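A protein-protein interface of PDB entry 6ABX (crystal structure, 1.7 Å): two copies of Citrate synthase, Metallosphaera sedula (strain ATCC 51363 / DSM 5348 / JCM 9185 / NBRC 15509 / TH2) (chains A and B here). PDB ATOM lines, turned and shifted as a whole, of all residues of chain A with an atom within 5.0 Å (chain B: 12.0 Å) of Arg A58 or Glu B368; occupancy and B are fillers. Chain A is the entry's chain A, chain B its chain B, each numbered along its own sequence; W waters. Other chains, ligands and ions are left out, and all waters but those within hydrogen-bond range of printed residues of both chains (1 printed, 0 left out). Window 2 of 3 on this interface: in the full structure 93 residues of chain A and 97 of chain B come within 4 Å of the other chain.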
ATOM      1  N   PRO A  56     -20.785   5.356 -19.817  1.00  0.00           N
ATOM      2  CA  PRO A  56     -21.494   4.608 -20.843  1.00  0.00           C
ATOM      3  C   PRO A  56     -21.002   3.166 -20.983  1.00  0.00           C
ATOM      4  O   PRO A  56     -19.842   2.905 -20.800  1.00  0.00           O
ATOM      5  CB  PRO A  56     -21.136   5.373 -22.123  1.00  0.00           C
ATOM      6  CG  PRO A  56     -19.762   5.916 -21.825  1.00  0.00           C
ATOM      7  CD  PRO A  56     -19.846   6.352 -20.376  1.00  0.00           C
ATOM      8  N   THR A  57     -21.890   2.288 -21.446  1.00  0.00           N
ATOM      9  CA  THR A  57     -21.407   0.990 -21.934  1.00  0.00           C
ATOM     10  C   THR A  57     -20.696   1.152 -23.270  1.00  0.00           C
ATOM     11  O   THR A  57     -20.712   2.184 -23.885  1.00  0.00           O
ATOM     12  CB  THR A  57     -22.564  -0.002 -22.083  1.00  0.00           C
ATOM     13  OG1 THR A  57     -23.387   0.495 -23.131  1.00  0.00           O
ATOM     14  CG2 THR A  57     -23.350  -0.141 -20.808  1.00  0.00           C
ATOM     15  N   ARG A  58     -20.011   0.087 -23.694  1.00  0.00           N
ATOM     16  CA  ARG A  58     -19.373   0.057 -24.977  1.00  0.00           C
ATOM     17  C   ARG A  58     -20.351   0.463 -26.099  1.00  0.00           C
ATOM     18  O   ARG A  58     -20.057   1.307 -26.932  1.00  0.00           O
ATOM     19  CB  ARG A  58     -18.774  -1.347 -25.170  1.00  0.00           C
ATOM     20  CG  ARG A  58     -17.894  -1.529 -26.393  1.00  0.00           C
ATOM     21  CD  ARG A  58     -17.260  -2.936 -26.297  1.00  0.00           C
ATOM     22  NE  ARG A  58     -17.431  -3.673 -27.534  1.00  0.00           N
ATOM     23  CZ  ARG A  58     -18.076  -4.819 -27.661  1.00  0.00           C
ATOM     24  NH1 ARG A  58     -18.316  -5.582 -26.608  1.00  0.00           N
ATOM     25  NH2 ARG A  58     -18.464  -5.203 -28.862  1.00  0.00           N
ATOM     26  N   HIS A  59     -21.540  -0.120 -26.136  1.00  0.00           N
ATOM     27  CA  HIS A  59     -22.521   0.193 -27.169  1.00  0.00           C
ATOM     28  C   HIS A  59     -23.007   1.644 -27.055  1.00  0.00           C
ATOM     29  O   HIS A  59     -23.161   2.311 -28.073  1.00  0.00           O
ATOM     30  CB  HIS A  59     -23.727  -0.761 -27.037  1.00  0.00           C
ATOM     31  CG  HIS A  59     -24.865  -0.471 -27.967  1.00  0.00           C
ATOM     32  ND1 HIS A  59     -26.069   0.059 -27.513  1.00  0.00           N
ATOM     33  CD2 HIS A  59     -25.023  -0.670 -29.303  1.00  0.00           C
ATOM     34  CE1 HIS A  59     -26.907   0.173 -28.535  1.00  0.00           C
ATOM     35  NE2 HIS A  59     -26.288  -0.268 -29.633  1.00  0.00           N
ATOM     36  N   GLU A  60     -23.276   2.113 -25.826  1.00  0.00           N
ATOM     37  CA  GLU A  60     -23.768   3.449 -25.627  1.00  0.00           C
ATOM     38  C   GLU A  60     -22.714   4.447 -26.122  1.00  0.00           C
ATOM     39  O   GLU A  60     -23.078   5.438 -26.807  1.00  0.00           O
ATOM     40  CB  GLU A  60     -24.097   3.733 -24.169  1.00  0.00           C
ATOM     41  CG  GLU A  60     -25.345   3.007 -23.687  1.00  0.00           C
ATOM     42  CD  GLU A  60     -25.547   3.065 -22.196  1.00  0.00           C
ATOM     43  OE1 GLU A  60     -24.566   3.254 -21.456  1.00  0.00           O
ATOM     44  OE2 GLU A  60     -26.706   2.962 -21.770  1.00  0.00           O
ATOM     45  N   LEU A  61     -21.442   4.151 -25.853  1.00  0.00           N
ATOM     46  CA  LEU A  61     -20.374   5.112 -26.212  1.00  0.00           C
ATOM     47  C   LEU A  61     -20.168   5.114 -27.734  1.00  0.00           C
ATOM     48  O   LEU A  61     -20.023   6.143 -28.330  1.00  0.00           O
ATOM     49  CB  LEU A  61     -19.082   4.802 -25.482  1.00  0.00           C
ATOM     50  CG  LEU A  61     -17.912   5.748 -25.779  1.00  0.00           C
ATOM     51  CD1 LEU A  61     -18.278   7.210 -25.552  1.00  0.00           C
ATOM     52  CD2 LEU A  61     -16.718   5.346 -24.930  1.00  0.00           C
ATOM     53  N   ASP A  62     -20.227   3.936 -28.351  1.00  0.00           N
ATOM     54  CA  ASP A  62     -20.116   3.809 -29.813  1.00  0.00           C
ATOM     55  C   ASP A  62     -21.215   4.617 -30.524  1.00  0.00           C
ATOM     56  O   ASP A  62     -20.954   5.350 -31.454  1.00  0.00           O
ATOM     57  CB  ASP A  62     -20.229   2.352 -30.260  1.00  0.00           C
ATOM     58  CG  ASP A  62     -19.865   2.216 -31.729  1.00  0.00           C
ATOM     59  OD1 ASP A  62     -18.706   2.602 -32.088  1.00  0.00           O
ATOM     60  OD2 ASP A  62     -20.746   1.810 -32.509  1.00  0.00           O
ATOM     61  N   ARG B 363     -15.046   4.782  -7.924  1.00  0.00           N
ATOM     62  CA  ARG B 363     -13.967   4.086  -8.617  1.00  0.00           C
ATOM     63  C   ARG B 363     -14.302   4.063 -10.116  1.00  0.00           C
ATOM     64  O   ARG B 363     -15.350   3.604 -10.498  1.00  0.00           O
ATOM     65  CB  ARG B 363     -13.788   2.639  -8.109  1.00  0.00           C
ATOM     66  CG  ARG B 363     -12.746   1.822  -8.868  1.00  0.00           C
ATOM     67  CD  ARG B 363     -12.629   0.338  -8.515  1.00  0.00           C
ATOM     68  NE  ARG B 363     -11.887  -0.436  -9.535  1.00  0.00           N
ATOM     69  CZ  ARG B 363     -10.582  -0.763  -9.491  1.00  0.00           C
ATOM     70  NH1 ARG B 363     -10.077  -1.649 -10.355  1.00  0.00           N
ATOM     71  NH2 ARG B 363      -9.788  -0.214  -8.580  1.00  0.00           N
ATOM     72  N   TYR B 364     -13.344   4.495 -10.939  1.00  0.00           N
ATOM     73  CA  TYR B 364     -13.453   4.445 -12.367  1.00  0.00           C
ATOM     74  C   TYR B 364     -13.363   2.986 -12.822  1.00  0.00           C
ATOM     75  O   TYR B 364     -12.441   2.272 -12.432  1.00  0.00           O
ATOM     76  CB  TYR B 364     -12.343   5.279 -13.017  1.00  0.00           C
ATOM     77  CG  TYR B 364     -12.436   5.246 -14.513  1.00  0.00           C
ATOM     78  CD1 TYR B 364     -13.238   6.159 -15.194  1.00  0.00           C
ATOM     79  CD2 TYR B 364     -11.735   4.333 -15.260  1.00  0.00           C
ATOM     80  CE1 TYR B 364     -13.403   6.091 -16.555  1.00  0.00           C
ATOM     81  CE2 TYR B 364     -11.885   4.247 -16.635  1.00  0.00           C
ATOM     82  CZ  TYR B 364     -12.643   5.201 -17.301  1.00  0.00           C
ATOM     83  OH  TYR B 364     -12.751   5.065 -18.638  1.00  0.00           O
ATOM     84  N   VAL B 365     -14.401   2.535 -13.540  1.00  0.00           N
ATOM     85  CA  VAL B 365     -14.505   1.201 -14.028  1.00  0.00           C
ATOM     86  C   VAL B 365     -14.238   1.308 -15.515  1.00  0.00           C
ATOM     87  O   VAL B 365     -14.881   2.097 -16.186  1.00  0.00           O
ATOM     88  CB  VAL B 365     -15.922   0.639 -13.826  1.00  0.00           C
ATOM     89  CG1 VAL B 365     -16.079  -0.753 -14.448  1.00  0.00           C
ATOM     90  CG2 VAL B 365     -16.308   0.605 -12.338  1.00  0.00           C
ATOM     91  N   PRO B 366     -13.271   0.584 -16.079  1.00  0.00           N
ATOM     92  CA  PRO B 366     -12.947   0.744 -17.502  1.00  0.00           C
ATOM     93  C   PRO B 366     -14.105   0.139 -18.304  1.00  0.00           C
ATOM     94  O   PRO B 366     -14.879  -0.696 -17.792  1.00  0.00           O
ATOM     95  CB  PRO B 366     -11.645  -0.044 -17.684  1.00  0.00           C
ATOM     96  CG  PRO B 366     -11.733  -1.072 -16.609  1.00  0.00           C
ATOM     97  CD  PRO B 366     -12.483  -0.477 -15.432  1.00  0.00           C
ATOM     98  N   ILE B 367     -14.205   0.533 -19.572  1.00  0.00           N
ATOM     99  CA  ILE B 367     -15.436   0.295 -20.300  1.00  0.00           C
ATOM    100  C   ILE B 367     -15.757  -1.197 -20.463  1.00  0.00           C
ATOM    101  O   ILE B 367     -16.937  -1.613 -20.434  1.00  0.00           O
ATOM    102  CB  ILE B 367     -15.421   1.107 -21.607  1.00  0.00           C
ATOM    103  CG1 ILE B 367     -16.846   1.199 -22.158  1.00  0.00           C
ATOM    104  CG2 ILE B 367     -14.418   0.604 -22.650  1.00  0.00           C
ATOM    105  CD1 ILE B 367     -17.013   2.233 -23.244  1.00  0.00           C
ATOM    106  N   GLU B 368     -14.721  -2.033 -20.599  1.00  0.00           N
ATOM    107  CA  GLU B 368     -14.967  -3.444 -20.842  1.00  0.00           C
ATOM    108  C   GLU B 368     -15.580  -4.127 -19.633  1.00  0.00           C
ATOM    109  O   GLU B 368     -16.154  -5.222 -19.787  1.00  0.00           O
ATOM    110  CB  GLU B 368     -13.693  -4.142 -21.286  1.00  0.00           C
ATOM    111  CG  GLU B 368     -13.268  -3.709 -22.658  1.00  0.00           C
ATOM    112  CD  GLU B 368     -14.027  -4.273 -23.858  1.00  0.00           C
ATOM    113  OE1 GLU B 368     -14.563  -3.460 -24.647  1.00  0.00           O
ATOM    114  OE2 GLU B 368     -14.017  -5.507 -24.058  1.00  0.00           O
ATOM    115  N   GLU B 369     -15.506  -3.505 -18.446  1.00  0.00           N
ATOM    116  CA  GLU B 369     -16.058  -4.057 -17.217  1.00  0.00           C
ATOM    117  C   GLU B 369     -17.462  -3.530 -16.900  1.00  0.00           C
ATOM    118  O   GLU B 369     -18.026  -3.937 -15.909  1.00  0.00           O
ATOM    119  CB  GLU B 369     -15.081  -3.783 -16.069  1.00  0.00           C
ATOM    120  CG  GLU B 369     -13.766  -4.527 -16.242  1.00  0.00           C
ATOM    121  CD  GLU B 369     -12.652  -4.259 -15.229  1.00  0.00           C
ATOM    122  OE1 GLU B 369     -12.953  -3.631 -14.248  1.00  0.00           O
ATOM    123  OE2 GLU B 369     -11.491  -4.686 -15.451  1.00  0.00           O
ATOM    124  N   ARG B 370     -18.000  -2.625 -17.723  1.00  0.00           N
ATOM    125  CA  ARG B 370     -19.347  -2.109 -17.590  1.00  0.00           C
ATOM    126  C   ARG B 370     -20.280  -3.005 -18.422  1.00  0.00           C
ATOM    127  O   ARG B 370     -21.015  -3.759 -17.826  1.00  0.00           O
ATOM    128  CB  ARG B 370     -19.406  -0.684 -18.120  1.00  0.00           C
ATOM    129  CG  ARG B 370     -18.343   0.225 -17.514  1.00  0.00           C
ATOM    130  CD  ARG B 370     -18.389   1.558 -18.217  1.00  0.00           C
ATOM    131  NE  ARG B 370     -17.243   2.360 -17.932  1.00  0.00           N
ATOM    132  CZ  ARG B 370     -16.712   3.257 -18.764  1.00  0.00           C
ATOM    133  NH1 ARG B 370     -17.407   3.710 -19.809  1.00  0.00           N
ATOM    134  NH2 ARG B 370     -15.499   3.702 -18.490  1.00  0.00           N
HETATM  135  O   HOH W   1     -19.254  -2.055 -21.717  1.00  0.00           O
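Water W1 bridges O of Ile B367 (2.7 Å) and N of Arg A58 (3.0 Å).
O of Pro A56 is in hydrogen-bond range of NH1 of Arg B370, at 2.7 Å.
Of chain A, only Arg A58 (3.2 Å) comes within 4 Å of Glu B368. Pro A56 touches two residues of chain B. Thr A57 touches just one residue of chain B: Ile B367. No residue of chain B comes within 4 Å of His A59. Of chain B, only Ile B367 (3.6 Å) comes within 4 Å of Leu A61. No residue of chain B comes within 4 Å of Asp A62. Of the printed residues of chain A, Arg B370 touches Pro A56 (2.7 Å). Of the printed residues of chain A, Ile B367 touches Pro A56, Thr A57, Arg A58 and Leu A61. Tyr B364 touches none of the printed residues of chain A. The nearest residue of chain B that does not touch Arg A58 is Arg B370 (5.7 Å).
Of the 8 printed residues of chain B, 3 touch a printed residue of chain A. Printed residues of chain B that touch a printed residue of chain A: Ile B367, Glu B368 and Arg B370. Hydrophobic or aromatic side chains of chain A that line the printed part of chain B: Pro A56 and Leu A61.
The backbone carbonyl oxygen of Val B365 lies within hydrogen-bond range of the guanidinium group of Arg B370 (2.9 Å). The side-chain hydroxyl (OH) of Tyr B364 is in hydrogen-bond range of the guanidinium group (NH2) of Arg B370 (3.1 Å). The side-chain carboxylate (OE1) of Glu A60 sits at hydrogen-bond distance from the backbone NH (N) of Thr A57, at 2.8 Å.
Pro A56 touches Ile B367 (O to CG1, 3.7 Å). Thr A57 touches Ile B367 (O to CD1, 3.8 Å). CD1 of Ile B367 touches CA of Arg A58, 3.6 Å away. Glu B368 touches Arg A58. CD2 of Leu A61 touches CD1 of Ile B367, 3.6 Å away.
No position is printed for both chains.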
